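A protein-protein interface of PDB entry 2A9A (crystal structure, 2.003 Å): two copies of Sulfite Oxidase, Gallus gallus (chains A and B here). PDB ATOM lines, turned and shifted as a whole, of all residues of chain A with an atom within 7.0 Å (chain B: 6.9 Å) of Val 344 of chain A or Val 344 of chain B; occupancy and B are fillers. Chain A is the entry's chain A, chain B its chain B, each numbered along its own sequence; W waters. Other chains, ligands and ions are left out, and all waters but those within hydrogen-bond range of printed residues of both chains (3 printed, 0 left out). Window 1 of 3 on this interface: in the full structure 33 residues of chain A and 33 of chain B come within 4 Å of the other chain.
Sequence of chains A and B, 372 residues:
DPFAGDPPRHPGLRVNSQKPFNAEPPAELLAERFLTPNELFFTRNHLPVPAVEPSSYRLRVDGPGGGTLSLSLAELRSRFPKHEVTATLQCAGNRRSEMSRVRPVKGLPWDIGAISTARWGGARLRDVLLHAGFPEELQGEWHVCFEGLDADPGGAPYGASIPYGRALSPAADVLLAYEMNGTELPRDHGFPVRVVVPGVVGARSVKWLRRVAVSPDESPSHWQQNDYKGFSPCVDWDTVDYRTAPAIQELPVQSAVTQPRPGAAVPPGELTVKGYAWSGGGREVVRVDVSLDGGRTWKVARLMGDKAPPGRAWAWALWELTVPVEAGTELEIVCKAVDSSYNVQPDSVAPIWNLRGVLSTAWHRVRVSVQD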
ATOM      1  N   PRO A 252      33.967  12.632 -11.164  1.00  0.00           N
ATOM      2  CA  PRO A 252      33.363  13.825 -10.566  1.00  0.00           C
ATOM      3  C   PRO A 252      33.512  13.937  -9.035  1.00  0.00           C
ATOM      4  O   PRO A 252      33.888  12.987  -8.379  1.00  0.00           O
ATOM      5  CB  PRO A 252      31.877  13.710 -10.968  1.00  0.00           C
ATOM      6  CG  PRO A 252      31.639  12.313 -11.219  1.00  0.00           C
ATOM      7  CD  PRO A 252      32.948  11.700 -11.670  1.00  0.00           C
ATOM      8  N   VAL A 253      33.241  15.114  -8.488  1.00  0.00           N
ATOM      9  CA  VAL A 253      33.317  15.351  -7.018  1.00  0.00           C
ATOM     10  C   VAL A 253      32.312  14.435  -6.269  1.00  0.00           C
ATOM     11  O   VAL A 253      31.210  14.160  -6.741  1.00  0.00           O
ATOM     12  CB  VAL A 253      33.195  16.885  -6.640  1.00  0.00           C
ATOM     13  CG1 VAL A 253      31.891  17.495  -7.118  1.00  0.00           C
ATOM     14  CG2 VAL A 253      33.323  17.079  -5.135  1.00  0.00           C
ATOM     15  N   GLN A 254      32.780  13.896  -5.145  1.00  0.00           N
ATOM     16  CA  GLN A 254      32.110  12.885  -4.391  1.00  0.00           C
ATOM     17  C   GLN A 254      32.344  13.075  -2.904  1.00  0.00           C
ATOM     18  O   GLN A 254      33.362  13.652  -2.484  1.00  0.00           O
ATOM     19  CB  GLN A 254      32.690  11.548  -4.841  1.00  0.00           C
ATOM     20  CG  GLN A 254      32.244  10.276  -4.098  1.00  0.00           C
ATOM     21  CD  GLN A 254      30.844   9.835  -4.464  1.00  0.00           C
ATOM     22  OE1 GLN A 254      30.641   8.888  -5.254  1.00  0.00           O
ATOM     23  NE2 GLN A 254      29.869  10.515  -3.902  1.00  0.00           N
ATOM     24  N   ARG A 287      35.673  22.643   0.086  1.00  0.00           N
ATOM     25  CA  ARG A 287      34.660  22.823   1.118  1.00  0.00           C
ATOM     26  C   ARG A 287      33.747  21.614   1.150  1.00  0.00           C
ATOM     27  O   ARG A 287      33.485  20.978   0.127  1.00  0.00           O
ATOM     28  CB  ARG A 287      33.842  24.109   0.865  1.00  0.00           C
ATOM     29  CG  ARG A 287      32.984  24.498   2.034  1.00  0.00           C
ATOM     30  CD  ARG A 287      32.193  25.730   1.802  1.00  0.00           C
ATOM     31  NE  ARG A 287      30.955  25.503   1.054  1.00  0.00           N
ATOM     32  CZ  ARG A 287      30.744  25.853  -0.218  1.00  0.00           C
ATOM     33  NH1 ARG A 287      31.643  26.539  -0.903  1.00  0.00           N
ATOM     34  NH2 ARG A 287      29.565  25.621  -0.769  1.00  0.00           N
ATOM     35  N   LYS A 336      27.807  17.353   1.105  1.00  0.00           N
ATOM     36  CA  LYS A 336      28.124  17.706  -0.256  1.00  0.00           C
ATOM     37  C   LYS A 336      29.446  18.461  -0.271  1.00  0.00           C
ATOM     38  O   LYS A 336      29.685  19.309   0.605  1.00  0.00           O
ATOM     39  CB  LYS A 336      26.952  18.476  -0.905  1.00  0.00           C
ATOM     40  CG  LYS A 336      26.637  19.861  -0.314  1.00  0.00           C
ATOM     41  CD  LYS A 336      25.371  20.431  -0.946  1.00  0.00           C
ATOM     42  CE  LYS A 336      25.054  21.793  -0.439  1.00  0.00           C
ATOM     43  NZ  LYS A 336      25.849  22.911  -0.989  1.00  0.00           N
ATOM     44  N   ALA A 337      30.297  18.123  -1.257  1.00  0.00           N
ATOM     45  CA  ALA A 337      31.608  18.674  -1.456  1.00  0.00           C
ATOM     46  C   ALA A 337      31.682  19.510  -2.725  1.00  0.00           C
ATOM     47  O   ALA A 337      30.847  19.345  -3.642  1.00  0.00           O
ATOM     48  CB  ALA A 337      32.653  17.582  -1.500  1.00  0.00           C
ATOM     49  N   VAL A 338      32.615  20.471  -2.667  1.00  0.00           N
ATOM     50  CA  VAL A 338      32.898  21.451  -3.721  1.00  0.00           C
ATOM     51  C   VAL A 338      34.392  21.321  -4.003  1.00  0.00           C
ATOM     52  O   VAL A 338      35.170  21.292  -3.037  1.00  0.00           O
ATOM     53  CB  VAL A 338      32.610  22.894  -3.249  1.00  0.00           C
ATOM     54  CG1 VAL A 338      32.824  23.889  -4.387  1.00  0.00           C
ATOM     55  CG2 VAL A 338      31.236  23.015  -2.707  1.00  0.00           C
ATOM     56  N   ASP A 339      34.794  21.202  -5.284  1.00  0.00           N
ATOM     57  CA  ASP A 339      36.202  21.061  -5.621  1.00  0.00           C
ATOM     58  C   ASP A 339      36.834  22.352  -6.141  1.00  0.00           C
ATOM     59  O   ASP A 339      36.179  23.412  -6.112  1.00  0.00           O
ATOM     60  CB  ASP A 339      36.461  19.860  -6.543  1.00  0.00           C
ATOM     61  CG  ASP A 339      36.134  20.134  -8.003  1.00  0.00           C
ATOM     62  OD1 ASP A 339      35.992  21.298  -8.365  1.00  0.00           O
ATOM     63  OD2 ASP A 339      36.110  19.170  -8.805  1.00  0.00           O
ATOM     64  N   SER A 341      37.705  23.485  -9.073  1.00  0.00           N
ATOM     65  CA  SER A 341      36.994  24.158 -10.212  1.00  0.00           C
ATOM     66  C   SER A 341      35.541  24.553  -9.868  1.00  0.00           C
ATOM     67  O   SER A 341      34.713  24.787 -10.763  1.00  0.00           O
ATOM     68  CB  SER A 341      36.937  23.245 -11.441  1.00  0.00           C
ATOM     69  OG  SER A 341      36.367  21.984 -11.060  1.00  0.00           O
ATOM     70  N   TYR A 342      35.217  24.555  -8.582  1.00  0.00           N
ATOM     71  CA  TYR A 342      33.874  24.797  -8.098  1.00  0.00           C
ATOM     72  C   TYR A 342      32.809  23.854  -8.702  1.00  0.00           C
ATOM     73  O   TYR A 342      31.632  24.169  -8.781  1.00  0.00           O
ATOM     74  CB  TYR A 342      33.545  26.287  -8.199  1.00  0.00           C
ATOM     75  CG  TYR A 342      34.194  27.133  -7.090  1.00  0.00           C
ATOM     76  CD1 TYR A 342      33.623  27.208  -5.823  1.00  0.00           C
ATOM     77  CD2 TYR A 342      35.375  27.813  -7.309  1.00  0.00           C
ATOM     78  CE1 TYR A 342      34.211  27.992  -4.815  1.00  0.00           C
ATOM     79  CE2 TYR A 342      35.948  28.613  -6.342  1.00  0.00           C
ATOM     80  CZ  TYR A 342      35.381  28.681  -5.077  1.00  0.00           C
ATOM     81  OH  TYR A 342      35.901  29.569  -4.153  1.00  0.00           O
ATOM     82  N   ASN A 343      33.213  22.619  -8.990  1.00  0.00           N
ATOM     83  CA  ASN A 343      32.231  21.609  -9.312  1.00  0.00           C
ATOM     84  C   ASN A 343      31.527  21.143  -8.015  1.00  0.00           C
ATOM     85  O   ASN A 343      32.145  21.118  -6.959  1.00  0.00           O
ATOM     86  CB  ASN A 343      32.839  20.446 -10.075  1.00  0.00           C
ATOM     87  CG  ASN A 343      32.981  20.748 -11.567  1.00  0.00           C
ATOM     88  OD1 ASN A 343      32.001  20.979 -12.262  1.00  0.00           O
ATOM     89  ND2 ASN A 343      34.214  20.781 -12.042  1.00  0.00           N
ATOM     90  N   VAL A 344      30.266  20.714  -8.153  1.00  0.00           N
ATOM     91  CA  VAL A 344      29.397  20.370  -7.055  1.00  0.00           C
ATOM     92  C   VAL A 344      28.634  19.058  -7.308  1.00  0.00           C
ATOM     93  O   VAL A 344      28.611  18.528  -8.416  1.00  0.00           O
ATOM     94  CB  VAL A 344      28.384  21.560  -6.785  1.00  0.00           C
ATOM     95  CG1 VAL A 344      29.103  22.806  -6.348  1.00  0.00           C
ATOM     96  CG2 VAL A 344      27.558  21.895  -8.013  1.00  0.00           C
ATOM     97  N   GLN A 345      28.088  18.505  -6.233  1.00  0.00           N
ATOM     98  CA  GLN A 345      27.266  17.319  -6.295  1.00  0.00           C
ATOM     99  C   GLN A 345      25.789  17.686  -6.523  1.00  0.00           C
ATOM    100  O   GLN A 345      25.248  18.658  -5.968  1.00  0.00           O
ATOM    101  CB  GLN A 345      27.433  16.474  -5.024  1.00  0.00           C
ATOM    102  CG  GLN A 345      28.834  15.951  -4.811  1.00  0.00           C
ATOM    103  CD  GLN A 345      28.998  15.171  -3.523  1.00  0.00           C
ATOM    104  OE1 GLN A 345      29.681  15.651  -2.587  1.00  0.00           O
ATOM    105  NE2 GLN A 345      28.262  14.038  -3.387  1.00  0.00           N
ATOM    106  N   PRO A 346      25.109  16.875  -7.356  1.00  0.00           N
ATOM    107  CA  PRO A 346      23.690  17.093  -7.571  1.00  0.00           C
ATOM    108  C   PRO A 346      22.842  16.638  -6.391  1.00  0.00           C
ATOM    109  O   PRO A 346      23.241  15.737  -5.645  1.00  0.00           O
ATOM    110  CB  PRO A 346      23.400  16.260  -8.811  1.00  0.00           C
ATOM    111  CG  PRO A 346      24.398  15.124  -8.783  1.00  0.00           C
ATOM    112  CD  PRO A 346      25.631  15.709  -8.107  1.00  0.00           C
ATOM    113  N   ILE A 352      20.595  11.589 -12.591  1.00  0.00           N
ATOM    114  CA  ILE A 352      21.901  11.038 -12.902  1.00  0.00           C
ATOM    115  C   ILE A 352      21.865   9.477 -13.008  1.00  0.00           C
ATOM    116  O   ILE A 352      22.922   8.833 -13.164  1.00  0.00           O
ATOM    117  CB  ILE A 352      23.008  11.455 -11.880  1.00  0.00           C
ATOM    118  CG1 ILE A 352      22.684  11.008 -10.451  1.00  0.00           C
ATOM    119  CG2 ILE A 352      23.306  12.976 -11.952  1.00  0.00           C
ATOM    120  CD1 ILE A 352      23.913  11.049  -9.559  1.00  0.00           C
ATOM    121  N   LEU A 359      28.859   6.233 -11.535  1.00  0.00           N
ATOM    122  CA  LEU A 359      28.840   7.702 -11.375  1.00  0.00           C
ATOM    123  C   LEU A 359      27.685   8.147 -10.482  1.00  0.00           C
ATOM    124  O   LEU A 359      26.812   8.966 -10.903  1.00  0.00           O
ATOM    125  CB  LEU A 359      28.746   8.376 -12.756  1.00  0.00           C
ATOM    126  CG  LEU A 359      29.894   8.097 -13.739  1.00  0.00           C
ATOM    127  CD1 LEU A 359      29.494   8.491 -15.124  1.00  0.00           C
ATOM    128  CD2 LEU A 359      31.153   8.816 -13.300  1.00  0.00           C
ATOM    129  N   THR A 361      26.891  10.064  -7.496  1.00  0.00           N
ATOM    130  CA  THR A 361      27.418  11.177  -6.672  1.00  0.00           C
ATOM    131  C   THR A 361      26.395  12.170  -6.122  1.00  0.00           C
ATOM    132  O   THR A 361      26.783  13.231  -5.607  1.00  0.00           O
ATOM    133  CB  THR A 361      28.451  12.028  -7.445  1.00  0.00           C
ATOM    134  OG1 THR A 361      27.828  12.683  -8.548  1.00  0.00           O
ATOM    135  CG2 THR A 361      29.575  11.207  -7.953  1.00  0.00           C
ATOM    136  N   TRP A 363      23.833  13.726  -3.330  1.00  0.00           N
ATOM    137  CA  TRP A 363      24.147  13.838  -1.897  1.00  0.00           C
ATOM    138  C   TRP A 363      23.795  12.595  -1.119  1.00  0.00           C
ATOM    139  O   TRP A 363      22.716  12.019  -1.290  1.00  0.00           O
ATOM    140  CB  TRP A 363      23.458  14.996  -1.183  1.00  0.00           C
ATOM    141  CG  TRP A 363      23.415  16.305  -1.939  1.00  0.00           C
ATOM    142  CD1 TRP A 363      24.320  16.767  -2.798  1.00  0.00           C
ATOM    143  CD2 TRP A 363      22.436  17.339  -1.781  1.00  0.00           C
ATOM    144  NE1 TRP A 363      23.910  17.983  -3.294  1.00  0.00           N
ATOM    145  CE2 TRP A 363      22.773  18.369  -2.661  1.00  0.00           C
ATOM    146  CE3 TRP A 363      21.284  17.460  -1.025  1.00  0.00           C
ATOM    147  CZ2 TRP A 363      22.014  19.537  -2.792  1.00  0.00           C
ATOM    148  CZ3 TRP A 363      20.514  18.625  -1.155  1.00  0.00           C
ATOM    149  CH2 TRP A 363      20.878  19.630  -2.037  1.00  0.00           C
ATOM    150  N   PRO B 252      32.746  25.593 -13.264  1.00  0.00           N
ATOM    151  CA  PRO B 252      32.061  24.307 -13.379  1.00  0.00           C
ATOM    152  C   PRO B 252      31.179  24.199 -14.653  1.00  0.00           C
ATOM    153  O   PRO B 252      30.978  25.175 -15.354  1.00  0.00           O
ATOM    154  CB  PRO B 252      31.234  24.263 -12.082  1.00  0.00           C
ATOM    155  CG  PRO B 252      30.989  25.671 -11.782  1.00  0.00           C
ATOM    156  CD  PRO B 252      32.172  26.430 -12.202  1.00  0.00           C
ATOM    157  N   VAL B 253      30.689  23.006 -14.938  1.00  0.00           N
ATOM    158  CA  VAL B 253      29.856  22.747 -16.106  1.00  0.00           C
ATOM    159  C   VAL B 253      28.571  23.599 -16.042  1.00  0.00           C
ATOM    160  O   VAL B 253      28.006  23.818 -14.970  1.00  0.00           O
ATOM    161  CB  VAL B 253      29.639  21.230 -16.330  1.00  0.00           C
ATOM    162  CG1 VAL B 253      28.979  20.548 -15.128  1.00  0.00           C
ATOM    163  CG2 VAL B 253      28.849  20.984 -17.603  1.00  0.00           C
ATOM    164  N   ARG B 287      27.598  15.604 -23.287  1.00  0.00           N
ATOM    165  CA  ARG B 287      26.181  15.351 -23.456  1.00  0.00           C
ATOM    166  C   ARG B 287      25.365  16.485 -22.858  1.00  0.00           C
ATOM    167  O   ARG B 287      25.790  17.193 -21.900  1.00  0.00           O
ATOM    168  CB  ARG B 287      25.769  14.012 -22.803  1.00  0.00           C
ATOM    169  CG  ARG B 287      24.489  13.422 -23.338  1.00  0.00           C
ATOM    170  CD  ARG B 287      24.108  12.136 -22.622  1.00  0.00           C
ATOM    171  NE  ARG B 287      23.630  12.333 -21.262  1.00  0.00           N
ATOM    172  CZ  ARG B 287      24.268  12.007 -20.128  1.00  0.00           C
ATOM    173  NH1 ARG B 287      25.424  11.353 -20.114  1.00  0.00           N
ATOM    174  NH2 ARG B 287      23.673  12.236 -18.963  1.00  0.00           N
ATOM    175  N   LYS B 336      20.493  20.188 -18.922  1.00  0.00           N
ATOM    176  CA  LYS B 336      21.639  19.982 -18.045  1.00  0.00           C
ATOM    177  C   LYS B 336      22.737  19.370 -18.879  1.00  0.00           C
ATOM    178  O   LYS B 336      22.458  18.538 -19.725  1.00  0.00           O
ATOM    179  CB  LYS B 336      21.236  19.122 -16.830  1.00  0.00           C
ATOM    180  CG  LYS B 336      20.788  17.712 -17.148  1.00  0.00           C
ATOM    181  CD  LYS B 336      20.260  17.004 -15.870  1.00  0.00           C
ATOM    182  CE  LYS B 336      19.774  15.589 -16.101  1.00  0.00           C
ATOM    183  NZ  LYS B 336      20.857  14.589 -16.399  1.00  0.00           N
ATOM    184  N   ALA B 337      23.987  19.698 -18.577  1.00  0.00           N
ATOM    185  CA  ALA B 337      25.121  19.222 -19.339  1.00  0.00           C
ATOM    186  C   ALA B 337      26.061  18.384 -18.467  1.00  0.00           C
ATOM    187  O   ALA B 337      26.068  18.508 -17.217  1.00  0.00           O
ATOM    188  CB  ALA B 337      25.858  20.403 -19.913  1.00  0.00           C
ATOM    189  N   VAL B 338      26.843  17.527 -19.143  1.00  0.00           N
ATOM    190  CA  VAL B 338      27.805  16.642 -18.521  1.00  0.00           C
ATOM    191  C   VAL B 338      29.119  16.902 -19.189  1.00  0.00           C
ATOM    192  O   VAL B 338      29.148  17.001 -20.400  1.00  0.00           O
ATOM    193  CB  VAL B 338      27.419  15.148 -18.727  1.00  0.00           C
ATOM    194  CG1 VAL B 338      28.475  14.221 -18.044  1.00  0.00           C
ATOM    195  CG2 VAL B 338      26.013  14.898 -18.208  1.00  0.00           C
ATOM    196  N   ASP B 339      30.207  17.047 -18.440  1.00  0.00           N
ATOM    197  CA  ASP B 339      31.540  17.283 -19.089  1.00  0.00           C
ATOM    198  C   ASP B 339      32.402  15.996 -19.202  1.00  0.00           C
ATOM    199  O   ASP B 339      31.918  14.882 -18.908  1.00  0.00           O
ATOM    200  CB  ASP B 339      32.281  18.509 -18.506  1.00  0.00           C
ATOM    201  CG  ASP B 339      32.985  18.260 -17.137  1.00  0.00           C
ATOM    202  OD1 ASP B 339      33.145  17.115 -16.679  1.00  0.00           O
ATOM    203  OD2 ASP B 339      33.416  19.269 -16.545  1.00  0.00           O
ATOM    204  N   SER B 341      34.945  14.953 -17.538  1.00  0.00           N
ATOM    205  CA  SER B 341      35.256  14.367 -16.243  1.00  0.00           C
ATOM    206  C   SER B 341      33.956  13.884 -15.559  1.00  0.00           C
ATOM    207  O   SER B 341      33.948  13.555 -14.390  1.00  0.00           O
ATOM    208  CB  SER B 341      35.907  15.409 -15.343  1.00  0.00           C
ATOM    209  OG  SER B 341      36.058  14.853 -14.024  1.00  0.00           O
ATOM    210  N   TYR B 342      32.865  13.895 -16.314  1.00  0.00           N
ATOM    211  CA  TYR B 342      31.533  13.521 -15.882  1.00  0.00           C
ATOM    212  C   TYR B 342      31.002  14.375 -14.731  1.00  0.00           C
ATOM    213  O   TYR B 342      30.250  13.895 -13.905  1.00  0.00           O
ATOM    214  CB  TYR B 342      31.432  12.004 -15.627  1.00  0.00           C
ATOM    215  CG  TYR B 342      31.280  11.188 -16.910  1.00  0.00           C
ATOM    216  CD1 TYR B 342      30.034  10.986 -17.486  1.00  0.00           C
ATOM    217  CD2 TYR B 342      32.379  10.543 -17.490  1.00  0.00           C
ATOM    218  CE1 TYR B 342      29.898  10.221 -18.658  1.00  0.00           C
ATOM    219  CE2 TYR B 342      32.269   9.828 -18.673  1.00  0.00           C
ATOM    220  CZ  TYR B 342      31.029   9.632 -19.233  1.00  0.00           C
ATOM    221  OH  TYR B 342      30.926   8.830 -20.334  1.00  0.00           O
ATOM    222  N   ASN B 343      31.475  15.616 -14.627  1.00  0.00           N
ATOM    223  CA  ASN B 343      30.878  16.574 -13.693  1.00  0.00           C
ATOM    224  C   ASN B 343      29.505  16.978 -14.285  1.00  0.00           C
ATOM    225  O   ASN B 343      29.306  16.950 -15.504  1.00  0.00           O
ATOM    226  CB  ASN B 343      31.825  17.742 -13.379  1.00  0.00           C
ATOM    227  CG  ASN B 343      32.712  17.452 -12.152  1.00  0.00           C
ATOM    228  OD1 ASN B 343      32.205  17.361 -11.025  1.00  0.00           O
ATOM    229  ND2 ASN B 343      34.012  17.215 -12.369  1.00  0.00           N
ATOM    230  N   VAL B 344      28.534  17.170 -13.391  1.00  0.00           N
ATOM    231  CA  VAL B 344      27.176  17.439 -13.709  1.00  0.00           C
ATOM    232  C   VAL B 344      26.664  18.662 -12.984  1.00  0.00           C
ATOM    233  O   VAL B 344      27.300  19.177 -12.060  1.00  0.00           O
ATOM    234  CB  VAL B 344      26.298  16.199 -13.350  1.00  0.00           C
ATOM    235  CG1 VAL B 344      26.768  15.010 -14.132  1.00  0.00           C
ATOM    236  CG2 VAL B 344      26.310  15.853 -11.844  1.00  0.00           C
ATOM    237  N   GLN B 345      25.537  19.172 -13.478  1.00  0.00           N
ATOM    238  CA  GLN B 345      24.834  20.335 -12.891  1.00  0.00           C
ATOM    239  C   GLN B 345      23.820  19.913 -11.822  1.00  0.00           C
ATOM    240  O   GLN B 345      23.131  18.879 -11.961  1.00  0.00           O
ATOM    241  CB  GLN B 345      24.089  21.116 -13.977  1.00  0.00           C
ATOM    242  CG  GLN B 345      24.981  21.813 -14.978  1.00  0.00           C
ATOM    243  CD  GLN B 345      24.202  22.546 -16.021  1.00  0.00           C
ATOM    244  OE1 GLN B 345      24.153  22.139 -17.173  1.00  0.00           O
ATOM    245  NE2 GLN B 345      23.603  23.660 -15.636  1.00  0.00           N
ATOM    246  N   PRO B 346      23.747  20.685 -10.734  1.00  0.00           N
ATOM    247  CA  PRO B 346      22.864  20.385  -9.638  1.00  0.00           C
ATOM    248  C   PRO B 346      21.438  20.729  -9.983  1.00  0.00           C
ATOM    249  O   PRO B 346      21.216  21.663 -10.747  1.00  0.00           O
ATOM    250  CB  PRO B 346      23.397  21.325  -8.515  1.00  0.00           C
ATOM    251  CG  PRO B 346      23.912  22.411  -9.178  1.00  0.00           C
ATOM    252  CD  PRO B 346      24.547  21.877 -10.433  1.00  0.00           C
ATOM    253  N   ILE B 352      23.139  25.883  -3.729  1.00  0.00           N
ATOM    254  CA  ILE B 352      24.374  26.534  -4.238  1.00  0.00           C
ATOM    255  C   ILE B 352      24.298  28.064  -4.076  1.00  0.00           C
ATOM    256  O   ILE B 352      25.094  28.784  -4.643  1.00  0.00           O
ATOM    257  CB  ILE B 352      24.712  26.183  -5.686  1.00  0.00           C
ATOM    258  CG1 ILE B 352      23.583  26.549  -6.661  1.00  0.00           C
ATOM    259  CG2 ILE B 352      25.043  24.708  -5.809  1.00  0.00           C
ATOM    260  CD1 ILE B 352      23.995  26.594  -8.101  1.00  0.00           C
ATOM    261  N   THR B 361      24.864  27.640 -11.589  1.00  0.00           N
ATOM    262  CA  THR B 361      24.878  26.531 -12.552  1.00  0.00           C
ATOM    263  C   THR B 361      23.824  25.464 -12.317  1.00  0.00           C
ATOM    264  O   THR B 361      23.895  24.431 -12.886  1.00  0.00           O
ATOM    265  CB  THR B 361      26.253  25.805 -12.619  1.00  0.00           C
ATOM    266  OG1 THR B 361      26.524  25.166 -11.376  1.00  0.00           O
ATOM    267  CG2 THR B 361      27.395  26.786 -13.001  1.00  0.00           C
ATOM    268  N   TRP B 363      20.148  23.653 -12.965  1.00  0.00           N
ATOM    269  CA  TRP B 363      19.439  23.517 -14.244  1.00  0.00           C
ATOM    270  C   TRP B 363      18.616  24.744 -14.606  1.00  0.00           C
ATOM    271  O   TRP B 363      17.891  25.316 -13.758  1.00  0.00           O
ATOM    272  CB  TRP B 363      18.475  22.316 -14.270  1.00  0.00           C
ATOM    273  CG  TRP B 363      18.994  21.031 -13.733  1.00  0.00           C
ATOM    274  CD1 TRP B 363      20.284  20.603 -13.755  1.00  0.00           C
ATOM    275  CD2 TRP B 363      18.223  19.952 -13.234  1.00  0.00           C
ATOM    276  NE1 TRP B 363      20.379  19.353 -13.217  1.00  0.00           N
ATOM    277  CE2 TRP B 363      19.113  18.894 -12.958  1.00  0.00           C
ATOM    278  CE3 TRP B 363      16.851  19.755 -13.014  1.00  0.00           C
ATOM    279  CZ2 TRP B 363      18.687  17.694 -12.398  1.00  0.00           C
ATOM    280  CZ3 TRP B 363      16.418  18.539 -12.481  1.00  0.00           C
ATOM    281  CH2 TRP B 363      17.325  17.537 -12.168  1.00  0.00           C
HETATM  282  O   HOH W   1      29.284  20.774 -11.160  1.00  0.00           O
HETATM  283  O   HOH W   2      29.767  17.103 -10.552  1.00  0.00           O
HETATM  284  O   HOH W   3      26.036  18.820  -9.605  1.00  0.00           O
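Water W2 lies within hydrogen-bond range of the side-chain amide oxygen of Asn 343 of chain B (2.5 Å), the backbone carbonyl oxygen of Val 344 of chain A (2.8 Å) and the backbone NH of Val 344 of chain B (3.1 Å).
Water W1 lies within hydrogen-bond range of O of Val 344 of chain B, OD1 of Asn 343 of chain A and N of Val 344 of chain A.
Water W3 bridges O of Val 344 of chain B (2.8 Å) and O of Val 344 of chain A (2.9 Å).
CB of Pro 252 of chain A touches O of Tyr 342 of chain B, 3.4 Å away.
CB of Pro 252 of chain A touches OD1 of Asn 343 of chain B, 3.7 Å away.
Val 253 of chain A touches Asn 343 of chain B (N to OD1, 3.5 Å).
Tyr 342 of chain A touches Pro 252 of chain B.
Asn 343 of chain A touches Val 253 of chain B (OD1 to N, 3.6 Å).
Asn 343 of chain B touches Asn 343 of chain A (OD1 to CB, 3.3 Å).
Val 344 of chain B touches Val 344 of chain A (O to O, 3.9 Å).
Val 344 of chain B touches Pro 346 of chain A (CG2 to CG, 3.7 Å).
Pro 346 of chain B touches Pro 346 of chain A (CA to CA, 3.97 Å).
Tyr 342 of chain B touches Leu 359 of chain A.
Of the 18 printed residues of chain A, 8 touch a printed residue of chain B.
Printed residues of chain A that touch a printed residue of chain B: Pro 252, Val 253, Ser 341, Tyr 342, Asn 343, Val 344, Pro 346 and Leu 359.
Hydrophobic or aromatic side chains of chain A that line the printed part of chain B: Pro 252, Val 253, Val 344, Pro 346 and Leu 359.
Along chain A the printed residues that touch a printed residue of chain B span positions 252 to 359.
Of the 16 printed residues of chain B, 7 touch a printed residue of chain A.
Along chain B the printed residues that touch a printed residue of chain A span positions 252 to 346.
Among the printed residues, 14 pairs touch across the chains.
Pro 252 of chain A touches Ser 341 of chain B, and with the chains exchanged Ser 341 of chain A touches Pro 252 of chain B.
Pro 252 of chain A touches Asn 343 of chain B, and with the chains exchanged Asn 343 of chain A touches Pro 252 of chain B.
Val 253 of chain A touches Asn 343 of chain B, and with the chains exchanged Asn 343 of chain A touches Val 253 of chain B.
Val 344 of chain B touches its own counterpart, Val 344 of chain A.
Positions printed for both chains: 252, 253, 287, 336, 337, 338, 339, 341, 342, 343, 344, 345, 346, 352, 361 and 363.
The side-chain hydroxyl (OG) of Ser 341 of chain A lies within hydrogen-bond range of the side-chain carboxylate (OD1) of Asp 339 of chain A (2.8 Å).
N of Tyr 342 of chain A sits at hydrogen-bond distance from OD1 of Asp 339 of chain A.
The side-chain carboxylate (OD1) of Asp 339 of chain B lies within hydrogen-bond range of the backbone NH (N) of Ser 341 of chain B, at 2.9 Å.
The side-chain carboxylate of Asp 339 of chain B sits at hydrogen-bond distance from the backbone NH of Tyr 342 of chain B (3.3 Å).
OD1 of Asp 339 of chain B sits at hydrogen-bond distance from N of Asn 343 of chain B (3.0 Å).
N of Trp 363 of chain B sits at hydrogen-bond distance from O of Pro 346 of chain B, at 3.2 Å.
The backbone nitrogen (N) of Pro 252 of chain A sits close to the backbone carbonyl oxygen (O) of Ser 341 of chain B.
The backbone carbonyl oxygen (O) of Ser 341 of chain A sits close to the backbone nitrogen (N) of Pro 252 of chain B, at 3.3 Å.
Printed residues of chain B within 4 Å of Val 344 of chain A: Val 344 and Pro 346.
Of the printed residues of chain B, Pro 346 of chain A touches Val 344 and Pro 346.
Of the printed residues of chain A, Val 253 of chain B touches Asn 343 (3.6 Å).
Printed residues of chain A within 4 Å of Val 344 of chain B: Val 344 (3.9 Å) and Pro 346 (3.7 Å).
The nearest residue of chain A that does not touch Val 344 of chain B is Ile 352 of chain A (4.2 Å).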
